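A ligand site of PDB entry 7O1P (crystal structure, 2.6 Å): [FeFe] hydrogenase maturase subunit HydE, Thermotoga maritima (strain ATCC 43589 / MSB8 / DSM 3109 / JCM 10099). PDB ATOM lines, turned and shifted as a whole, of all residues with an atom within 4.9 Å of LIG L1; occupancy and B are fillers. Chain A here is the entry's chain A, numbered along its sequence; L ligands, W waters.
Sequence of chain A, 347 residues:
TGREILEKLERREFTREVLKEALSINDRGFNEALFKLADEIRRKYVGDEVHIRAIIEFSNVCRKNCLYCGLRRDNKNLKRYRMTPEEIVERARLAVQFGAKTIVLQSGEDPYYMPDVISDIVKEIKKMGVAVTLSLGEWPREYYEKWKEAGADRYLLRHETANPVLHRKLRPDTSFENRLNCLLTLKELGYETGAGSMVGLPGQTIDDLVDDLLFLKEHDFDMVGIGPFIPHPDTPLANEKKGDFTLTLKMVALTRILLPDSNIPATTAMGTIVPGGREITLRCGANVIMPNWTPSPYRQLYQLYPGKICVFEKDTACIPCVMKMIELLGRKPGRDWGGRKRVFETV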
ATOM      1  N   CYS A  62       1.862 -13.267 -10.258  1.00  0.00           N
ATOM      2  CA  CYS A  62       2.278 -12.045 -10.918  1.00  0.00           C
ATOM      3  C   CYS A  62       1.203 -11.538 -11.873  1.00  0.00           C
ATOM      4  O   CYS A  62       0.485 -12.323 -12.498  1.00  0.00           O
ATOM      5  CB  CYS A  62       3.589 -12.221 -11.680  1.00  0.00           C
ATOM      6  SG  CYS A  62       4.277 -10.654 -12.251  1.00  0.00           S
ATOM      7  N   TYR A  68      10.147 -13.838 -20.904  1.00  0.00           N
ATOM      8  CA  TYR A  68      11.181 -14.755 -20.413  1.00  0.00           C
ATOM      9  C   TYR A  68      10.776 -15.469 -19.129  1.00  0.00           C
ATOM     10  O   TYR A  68      11.277 -16.572 -18.881  1.00  0.00           O
ATOM     11  CB  TYR A  68      12.485 -13.988 -20.173  1.00  0.00           C
ATOM     12  CG  TYR A  68      12.290 -12.682 -19.402  1.00  0.00           C
ATOM     13  CD1 TYR A  68      12.253 -12.680 -18.012  1.00  0.00           C
ATOM     14  CD2 TYR A  68      12.134 -11.479 -20.079  1.00  0.00           C
ATOM     15  CE1 TYR A  68      12.071 -11.499 -17.312  1.00  0.00           C
ATOM     16  CE2 TYR A  68      11.957 -10.297 -19.393  1.00  0.00           C
ATOM     17  CZ  TYR A  68      11.923 -10.308 -18.003  1.00  0.00           C
ATOM     18  OH  TYR A  68      11.750  -9.132 -17.323  1.00  0.00           O
ATOM     19  N   CYS A  69       9.895 -14.886 -18.326  1.00  0.00           N
ATOM     20  CA  CYS A  69       9.683 -15.332 -16.962  1.00  0.00           C
ATOM     21  C   CYS A  69       8.597 -16.405 -16.884  1.00  0.00           C
ATOM     22  O   CYS A  69       7.546 -16.295 -17.513  1.00  0.00           O
ATOM     23  CB  CYS A  69       9.290 -14.156 -16.061  1.00  0.00           C
ATOM     24  SG  CYS A  69       9.124 -14.608 -14.338  1.00  0.00           S
ATOM     25  N   GLN A 106      10.973 -11.051  -2.027  1.00  0.00           N
ATOM     26  CA  GLN A 106      10.774 -11.000  -3.461  1.00  0.00           C
ATOM     27  C   GLN A 106       9.546 -11.811  -3.838  1.00  0.00           C
ATOM     28  O   GLN A 106       9.239 -12.824  -3.212  1.00  0.00           O
ATOM     29  CB  GLN A 106      11.985 -11.541  -4.235  1.00  0.00           C
ATOM     30  CG  GLN A 106      11.856 -11.428  -5.742  1.00  0.00           C
ATOM     31  CD  GLN A 106      13.018 -12.062  -6.476  1.00  0.00           C
ATOM     32  OE1 GLN A 106      13.141 -13.290  -6.505  1.00  0.00           O
ATOM     33  NE2 GLN A 106      13.867 -11.248  -7.082  1.00  0.00           N
ATOM     34  N   SER A 107       8.854 -11.349  -4.876  1.00  0.00           N
ATOM     35  CA  SER A 107       7.684 -12.047  -5.408  1.00  0.00           C
ATOM     36  C   SER A 107       7.418 -11.525  -6.804  1.00  0.00           C
ATOM     37  O   SER A 107       8.007 -10.530  -7.244  1.00  0.00           O
ATOM     38  CB  SER A 107       6.454 -11.833  -4.513  1.00  0.00           C
ATOM     39  OG  SER A 107       6.083 -10.468  -4.492  1.00  0.00           O
ATOM     40  N   GLY A 108       6.531 -12.210  -7.503  1.00  0.00           N
ATOM     41  CA  GLY A 108       5.883 -11.597  -8.652  1.00  0.00           C
ATOM     42  C   GLY A 108       5.046 -10.419  -8.211  1.00  0.00           C
ATOM     43  O   GLY A 108       4.808 -10.197  -7.021  1.00  0.00           O
ATOM     44  N   GLU A 109       4.597  -9.640  -9.183  1.00  0.00           N
ATOM     45  CA  GLU A 109       3.779  -8.476  -8.866  1.00  0.00           C
ATOM     46  C   GLU A 109       2.396  -8.925  -8.423  1.00  0.00           C
ATOM     47  O   GLU A 109       1.495  -9.094  -9.241  1.00  0.00           O
ATOM     48  CB  GLU A 109       3.701  -7.530 -10.060  1.00  0.00           C
ATOM     49  CG  GLU A 109       5.065  -7.055 -10.552  1.00  0.00           C
ATOM     50  CD  GLU A 109       5.004  -5.775 -11.344  1.00  0.00           C
ATOM     51  OE1 GLU A 109       3.899  -5.371 -11.753  1.00  0.00           O
ATOM     52  OE2 GLU A 109       6.075  -5.152 -11.541  1.00  0.00           O
ATOM     53  N   SER A 135      12.002  -6.664  -3.311  1.00  0.00           N
ATOM     54  CA  SER A 135      12.119  -6.945  -4.742  1.00  0.00           C
ATOM     55  C   SER A 135      10.720  -7.327  -5.239  1.00  0.00           C
ATOM     56  O   SER A 135      10.389  -8.506  -5.424  1.00  0.00           O
ATOM     57  CB  SER A 135      13.144  -8.046  -5.036  1.00  0.00           C
ATOM     58  OG  SER A 135      13.213  -8.347  -6.419  1.00  0.00           O
ATOM     59  N   LEU A 136       9.882  -6.320  -5.472  1.00  0.00           N
ATOM     60  CA  LEU A 136       8.462  -6.532  -5.736  1.00  0.00           C
ATOM     61  C   LEU A 136       8.028  -5.979  -7.085  1.00  0.00           C
ATOM     62  O   LEU A 136       6.832  -5.963  -7.377  1.00  0.00           O
ATOM     63  CB  LEU A 136       7.615  -5.907  -4.627  1.00  0.00           C
ATOM     64  CG  LEU A 136       7.976  -6.255  -3.183  1.00  0.00           C
ATOM     65  CD1 LEU A 136       6.999  -5.619  -2.220  1.00  0.00           C
ATOM     66  CD2 LEU A 136       8.039  -7.757  -2.985  1.00  0.00           C
ATOM     67  N   GLY A 137       8.961  -5.531  -7.915  1.00  0.00           N
ATOM     68  CA  GLY A 137       8.604  -5.012  -9.217  1.00  0.00           C
ATOM     69  C   GLY A 137       8.219  -3.548  -9.190  1.00  0.00           C
ATOM     70  O   GLY A 137       8.610  -2.791  -8.281  1.00  0.00           O
ATOM     71  N   LEU A 157      15.514  -3.988  -8.371  1.00  0.00           N
ATOM     72  CA  LEU A 157      14.673  -3.826  -9.553  1.00  0.00           C
ATOM     73  C   LEU A 157      15.624  -3.821 -10.755  1.00  0.00           C
ATOM     74  O   LEU A 157      16.016  -2.769 -11.260  1.00  0.00           O
ATOM     75  CB  LEU A 157      13.849  -2.540  -9.483  1.00  0.00           C
ATOM     76  CG  LEU A 157      12.827  -2.329 -10.597  1.00  0.00           C
ATOM     77  CD1 LEU A 157      11.489  -2.934 -10.209  1.00  0.00           C
ATOM     78  CD2 LEU A 157      12.693  -0.848 -10.907  1.00  0.00           C
ATOM     79  N   ARG A 158      16.000  -5.021 -11.187  1.00  0.00           N
ATOM     80  CA  ARG A 158      16.901  -5.154 -12.325  1.00  0.00           C
ATOM     81  C   ARG A 158      16.334  -4.447 -13.539  1.00  0.00           C
ATOM     82  O   ARG A 158      15.136  -4.555 -13.838  1.00  0.00           O
ATOM     83  CB  ARG A 158      17.143  -6.628 -12.649  1.00  0.00           C
ATOM     84  CG  ARG A 158      17.996  -7.400 -11.648  1.00  0.00           C
ATOM     85  CD  ARG A 158      18.316  -8.769 -12.227  1.00  0.00           C
ATOM     86  NE  ARG A 158      18.812  -9.712 -11.227  1.00  0.00           N
ATOM     87  CZ  ARG A 158      18.914 -11.019 -11.432  1.00  0.00           C
ATOM     88  NH1 ARG A 158      18.550 -11.538 -12.599  1.00  0.00           N
ATOM     89  NH2 ARG A 158      19.374 -11.817 -10.481  1.00  0.00           N
ATOM     90  N   GLU A 160      16.973  -5.214 -16.502  1.00  0.00           N
ATOM     91  CA  GLU A 160      16.706  -6.305 -17.449  1.00  0.00           C
ATOM     92  C   GLU A 160      17.415  -6.113 -18.787  1.00  0.00           C
ATOM     93  O   GLU A 160      18.097  -7.029 -19.263  1.00  0.00           O
ATOM     94  CB  GLU A 160      15.196  -6.460 -17.657  1.00  0.00           C
ATOM     95  CG  GLU A 160      14.343  -6.459 -16.373  1.00  0.00           C
ATOM     96  CD  GLU A 160      14.515  -7.694 -15.497  1.00  0.00           C
ATOM     97  OE1 GLU A 160      15.511  -8.441 -15.669  1.00  0.00           O
ATOM     98  OE2 GLU A 160      13.649  -7.931 -14.625  1.00  0.00           O
ATOM     99  N   ARG A 171       8.996  -7.200 -22.327  1.00  0.00           N
ATOM    100  CA  ARG A 171       8.108  -6.882 -21.216  1.00  0.00           C
ATOM    101  C   ARG A 171       6.979  -6.036 -21.788  1.00  0.00           C
ATOM    102  O   ARG A 171       7.064  -4.808 -21.841  1.00  0.00           O
ATOM    103  CB  ARG A 171       8.878  -6.165 -20.103  1.00  0.00           C
ATOM    104  CG  ARG A 171      10.243  -6.794 -19.835  1.00  0.00           C
ATOM    105  CD  ARG A 171      10.921  -6.217 -18.605  1.00  0.00           C
ATOM    106  NE  ARG A 171      10.186  -6.521 -17.388  1.00  0.00           N
ATOM    107  CZ  ARG A 171       9.731  -5.598 -16.547  1.00  0.00           C
ATOM    108  NH1 ARG A 171       9.947  -4.312 -16.795  1.00  0.00           N
ATOM    109  NH2 ARG A 171       9.061  -5.955 -15.464  1.00  0.00           N
ATOM    110  N   ARG A 179      10.649   1.522 -16.173  1.00  0.00           N
ATOM    111  CA  ARG A 179      11.615   0.825 -15.333  1.00  0.00           C
ATOM    112  C   ARG A 179      12.705   1.768 -14.848  1.00  0.00           C
ATOM    113  O   ARG A 179      13.083   1.751 -13.662  1.00  0.00           O
ATOM    114  CB  ARG A 179      12.225  -0.346 -16.092  1.00  0.00           C
ATOM    115  CG  ARG A 179      12.899  -1.396 -15.228  1.00  0.00           C
ATOM    116  CD  ARG A 179      11.880  -2.345 -14.617  1.00  0.00           C
ATOM    117  NE  ARG A 179      12.497  -3.525 -14.009  1.00  0.00           N
ATOM    118  CZ  ARG A 179      11.823  -4.480 -13.376  1.00  0.00           C
ATOM    119  NH1 ARG A 179      10.504  -4.389 -13.265  1.00  0.00           N
ATOM    120  NH2 ARG A 179      12.461  -5.507 -12.849  1.00  0.00           N
ATOM    121  N   MET A 198      19.830  -9.399 -17.604  1.00  0.00           N
ATOM    122  CA  MET A 198      20.098 -10.755 -18.034  1.00  0.00           C
ATOM    123  C   MET A 198      21.049 -10.736 -19.218  1.00  0.00           C
ATOM    124  O   MET A 198      21.117  -9.761 -19.968  1.00  0.00           O
ATOM    125  CB  MET A 198      18.796 -11.482 -18.413  1.00  0.00           C
ATOM    126  CG  MET A 198      17.972 -11.929 -17.223  1.00  0.00           C
ATOM    127  SD  MET A 198      16.360 -12.581 -17.694  1.00  0.00           S
ATOM    128  CE  MET A 198      15.485 -11.062 -18.070  1.00  0.00           C
ATOM    129  N   PRO A 228      22.516 -15.339 -16.401  1.00  0.00           N
ATOM    130  CA  PRO A 228      22.242 -15.801 -17.771  1.00  0.00           C
ATOM    131  C   PRO A 228      20.759 -16.016 -17.983  1.00  0.00           C
ATOM    132  O   PRO A 228      20.033 -16.439 -17.081  1.00  0.00           O
ATOM    133  CB  PRO A 228      23.008 -17.130 -17.838  1.00  0.00           C
ATOM    134  CG  PRO A 228      22.946 -17.643 -16.425  1.00  0.00           C
ATOM    135  CD  PRO A 228      23.071 -16.409 -15.560  1.00  0.00           C
ATOM    136  N   PHE A 229      20.294 -15.713 -19.199  1.00  0.00           N
ATOM    137  CA  PHE A 229      18.918 -16.015 -19.548  1.00  0.00           C
ATOM    138  C   PHE A 229      18.715 -17.530 -19.588  1.00  0.00           C
ATOM    139  O   PHE A 229      19.438 -18.241 -20.282  1.00  0.00           O
ATOM    140  CB  PHE A 229      18.544 -15.397 -20.891  1.00  0.00           C
ATOM    141  CG  PHE A 229      17.320 -16.011 -21.501  1.00  0.00           C
ATOM    142  CD1 PHE A 229      16.082 -15.856 -20.911  1.00  0.00           C
ATOM    143  CD2 PHE A 229      17.404 -16.743 -22.678  1.00  0.00           C
ATOM    144  CE1 PHE A 229      14.947 -16.414 -21.474  1.00  0.00           C
ATOM    145  CE2 PHE A 229      16.272 -17.315 -23.242  1.00  0.00           C
ATOM    146  CZ  PHE A 229      15.045 -17.143 -22.631  1.00  0.00           C
ATOM    147  N   ILE A 230      17.740 -18.008 -18.830  1.00  0.00           N
ATOM    148  CA  ILE A 230      17.409 -19.432 -18.823  1.00  0.00           C
ATOM    149  C   ILE A 230      15.981 -19.595 -19.343  1.00  0.00           C
ATOM    150  O   ILE A 230      15.030 -19.141 -18.703  1.00  0.00           O
ATOM    151  CB  ILE A 230      17.586 -20.040 -17.432  1.00  0.00           C
ATOM    152  CG1 ILE A 230      19.029 -19.864 -16.958  1.00  0.00           C
ATOM    153  CG2 ILE A 230      17.184 -21.509 -17.441  1.00  0.00           C
ATOM    154  CD1 ILE A 230      19.310 -20.476 -15.604  1.00  0.00           C
ATOM    155  N   PRO A 231      15.804 -20.229 -20.500  1.00  0.00           N
ATOM    156  CA  PRO A 231      14.451 -20.374 -21.050  1.00  0.00           C
ATOM    157  C   PRO A 231      13.568 -21.249 -20.160  1.00  0.00           C
ATOM    158  O   PRO A 231      14.018 -22.255 -19.617  1.00  0.00           O
ATOM    159  CB  PRO A 231      14.690 -21.020 -22.418  1.00  0.00           C
ATOM    160  CG  PRO A 231      16.023 -21.697 -22.289  1.00  0.00           C
ATOM    161  CD  PRO A 231      16.825 -20.821 -21.373  1.00  0.00           C
ATOM    162  N   ALA A 269      21.148 -18.368 -11.001  1.00  0.00           N
ATOM    163  CA  ALA A 269      21.153 -18.726 -12.415  1.00  0.00           C
ATOM    164  C   ALA A 269      22.535 -19.149 -12.883  1.00  0.00           C
ATOM    165  O   ALA A 269      22.675 -20.037 -13.724  1.00  0.00           O
ATOM    166  CB  ALA A 269      20.634 -17.561 -13.261  1.00  0.00           C
ATOM    167  N   TYR A 302       8.306 -21.527  -7.373  1.00  0.00           N
ATOM    168  CA  TYR A 302       8.767 -20.186  -7.744  1.00  0.00           C
ATOM    169  C   TYR A 302       9.753 -20.327  -8.896  1.00  0.00           C
ATOM    170  O   TYR A 302      10.974 -20.297  -8.720  1.00  0.00           O
ATOM    171  CB  TYR A 302       9.384 -19.493  -6.538  1.00  0.00           C
ATOM    172  CG  TYR A 302       9.612 -18.008  -6.736  1.00  0.00           C
ATOM    173  CD1 TYR A 302       8.616 -17.090  -6.438  1.00  0.00           C
ATOM    174  CD2 TYR A 302      10.823 -17.534  -7.201  1.00  0.00           C
ATOM    175  CE1 TYR A 302       8.822 -15.734  -6.621  1.00  0.00           C
ATOM    176  CE2 TYR A 302      11.039 -16.176  -7.380  1.00  0.00           C
ATOM    177  CZ  TYR A 302      10.036 -15.281  -7.080  1.00  0.00           C
ATOM    178  OH  TYR A 302      10.242 -13.933  -7.256  1.00  0.00           O
ATOM    179  N   LEU A 304      10.923 -18.591 -11.879  1.00  0.00           N
ATOM    180  CA  LEU A 304      11.323 -17.632 -12.901  1.00  0.00           C
ATOM    181  C   LEU A 304      11.937 -18.361 -14.086  1.00  0.00           C
ATOM    182  O   LEU A 304      11.603 -18.102 -15.242  1.00  0.00           O
ATOM    183  CB  LEU A 304      12.314 -16.621 -12.316  1.00  0.00           C
ATOM    184  CG  LEU A 304      11.965 -15.993 -10.969  1.00  0.00           C
ATOM    185  CD1 LEU A 304      13.173 -15.272 -10.405  1.00  0.00           C
ATOM    186  CD2 LEU A 304      10.778 -15.050 -11.088  1.00  0.00           C
ATOM    187  N   TYR A 305      12.811 -19.312 -13.780  1.00  0.00           N
ATOM    188  CA  TYR A 305      13.432 -20.258 -14.692  1.00  0.00           C
ATOM    189  C   TYR A 305      13.417 -21.605 -13.974  1.00  0.00           C
ATOM    190  O   TYR A 305      13.176 -21.653 -12.764  1.00  0.00           O
ATOM    191  CB  TYR A 305      14.866 -19.822 -15.033  1.00  0.00           C
ATOM    192  CG  TYR A 305      15.718 -19.560 -13.813  1.00  0.00           C
ATOM    193  CD1 TYR A 305      16.426 -20.580 -13.190  1.00  0.00           C
ATOM    194  CD2 TYR A 305      15.831 -18.276 -13.280  1.00  0.00           C
ATOM    195  CE1 TYR A 305      17.205 -20.347 -12.076  1.00  0.00           C
ATOM    196  CE2 TYR A 305      16.612 -18.035 -12.172  1.00  0.00           C
ATOM    197  CZ  TYR A 305      17.301 -19.074 -11.574  1.00  0.00           C
ATOM    198  OH  TYR A 305      18.073 -18.828 -10.476  1.00  0.00           O
HETATM  199  N1  LIG L   1       8.581  -9.507 -10.341  1.00  0.00           N
HETATM  200  C1  LIG L   1       9.713  -8.737  -9.838  1.00  0.00           C
HETATM  201  C2  LIG L   1      10.632  -9.605  -8.975  1.00  0.00           C
HETATM  202  C3  LIG L   1      10.936 -11.024  -9.460  1.00  0.00           C
HETATM  203  S1  LIG L   1      11.646 -11.150 -11.115  1.00  0.00           S
HETATM  204  C4  LIG L   1      10.503  -8.118 -10.983  1.00  0.00           C
HETATM  205  O1  LIG L   1      10.257  -8.419 -12.156  1.00  0.00           O
HETATM  206  O2  LIG L   1      11.419  -7.318 -10.754  1.00  0.00           O
HETATM  207  C5  LIG L   1      13.307 -11.351 -10.422  1.00  0.00           C
HETATM  208  C6  LIG L   1      14.398 -11.448 -11.477  1.00  0.00           C
HETATM  209  O3  LIG L   1      14.512 -12.751 -12.019  1.00  0.00           O
HETATM  210  C7  LIG L   1      14.159 -10.533 -12.666  1.00  0.00           C
HETATM  211  O4  LIG L   1      14.762  -9.284 -12.456  1.00  0.00           O
HETATM  212  C8  LIG L   1      14.814 -11.262 -13.813  1.00  0.00           C
HETATM  213  O5  LIG L   1      16.027 -10.637 -14.176  1.00  0.00           O
HETATM  214  C9  LIG L   1      15.127 -12.649 -13.289  1.00  0.00           C
HETATM  215  N2  LIG L   1      14.612 -13.645 -14.249  1.00  0.00           N
HETATM  216  C10 LIG L   1      13.299 -13.838 -14.570  1.00  0.00           C
HETATM  217  N3  LIG L   1      13.229 -14.824 -15.493  1.00  0.00           N
HETATM  218  C11 LIG L   1      14.480 -15.254 -15.768  1.00  0.00           C
HETATM  219  C12 LIG L   1      14.967 -16.227 -16.633  1.00  0.00           C
HETATM  220  N4  LIG L   1      14.133 -16.941 -17.392  1.00  0.00           N
HETATM  221  N5  LIG L   1      16.323 -16.448 -16.709  1.00  0.00           N
HETATM  222  C13 LIG L   1      17.191 -15.712 -15.936  1.00  0.00           C
HETATM  223  N6  LIG L   1      16.695 -14.742 -15.074  1.00  0.00           N
HETATM  224  C14 LIG L   1      15.366 -14.514 -14.988  1.00  0.00           C
HETATM  225 FE1  LG2 L   2       8.447 -12.498 -13.889  1.00  0.00          FE
HETATM  226 FE2  LG2 L   2       6.374 -10.961 -13.116  1.00  0.00          FE
HETATM  227 FE3  LG2 L   2       8.034 -10.070 -15.028  1.00  0.00          FE
HETATM  228 FE4  LG2 L   2       8.865 -10.218 -12.391  1.00  0.00          FE
HETATM  229  S1  LG2 L   2       7.246  -8.839 -13.250  1.00  0.00           S
HETATM  230  S2  LG2 L   2      10.042 -10.882 -14.253  1.00  0.00           S
HETATM  231  S3  LG2 L   2       7.784 -12.128 -11.717  1.00  0.00           S
HETATM  232  S4  LG2 L   2       6.646 -11.907 -15.196  1.00  0.00           S
HETATM  233  O   HOH W   1      14.691  -7.221 -10.436  1.00  0.00           O
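An oxygen (O5) of LIG L1 lies within hydrogen-bond range of the side-chain carboxylate (OE1) of Glu 160 (2.7 Å). N5 of LIG L1 sits at hydrogen-bond distance from N of Ile 230 (3.0 Å). O of Ile 230 sits at hydrogen-bond distance from N4 of LIG L1 (2.7 Å). The guanidinium group (NH2) of Arg 179 lies within salt-bridge range of an oxygen (O2) of LIG L1, 3.0 Å away. NH1 of Arg 158 sits at hydrogen-bond distance from O5 of LIG L1 (3.1 Å). N4 of LIG L1 sits at hydrogen-bond distance from O of Tyr 68 (3.2 Å). The backbone carbonyl oxygen of Ser 107 sits close to a nitrogen (N1) of LIG L1 (3.3 Å). The side-chain sulfur (SG) of Cys 69 is bound to an iron atom (FE1) of LG2 L2, 2.3 Å away. An iron atom (FE2) of LG2 L2 is bound by the side-chain sulfur (SG) of Cys 62 (2.3 Å).
N1 of LIG L1 is bound to FE4 of LG2 L2 (2.2 Å).
The side-chain sulfur (SD) of Met 198 sits close to a nitrogen (N6) of LIG L1, 3.4 Å away. CA of Cys 69 touches N3 of LIG L1 (3.9 Å). NE2 of Gln 106 touches C5 of LIG L1 (3.4 Å). CA of Gly 108 touches N1 of LIG L1, at 3.8 Å. O of Ser 135 touches C2 of LIG L1, at 3.7 Å. Gly 137 touches LIG L1. Pro 228 touches LIG L1 (O to C13, 3.1 Å). CA of Phe 229 touches N5 of LIG L1, at 3.9 Å. Tyr 302 touches LIG L1. Leu 304 touches LIG L1. Tyr 305 touches LIG L1 (CB to N4, 3.8 Å). The nearest printed residue that does not touch LIG L1 is Glu 109 (4.2 Å).
Water W1 bridges N of Arg 158 (2.7 Å) and O4 of LIG L1 (2.9 Å).
NH2 of Arg 179 is in salt-bridge range of OE2 of Glu 160 (3.2 Å). The backbone NH of Met 198 lies within hydrogen-bond range of the backbone carbonyl oxygen of Glu 160 (3.4 Å). The guanidinium group (NE) of Arg 179 sits at hydrogen-bond distance from the backbone carbonyl oxygen (O) of Arg 158 (2.8 Å). The guanidinium group (NE) of Arg 171 lies within hydrogen-bond range of the side-chain hydroxyl (OH) of Tyr 68, at 3.0 Å. The backbone NH (N) of Ser 107 is in hydrogen-bond range of the backbone carbonyl oxygen (O) of Ser 135 (3.3 Å). The side-chain amide oxygen (OE1) of Gln 106 lies within hydrogen-bond range of the side-chain hydroxyl (OH) of Tyr 302. The side-chain hydroxyl of Ser 135 is in hydrogen-bond range of the side-chain amide nitrogen of Gln 106, 3.0 Å away. The backbone NH (N) of Ala 269 is in hydrogen-bond range of the side-chain hydroxyl (OH) of Tyr 305 (3.2 Å).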
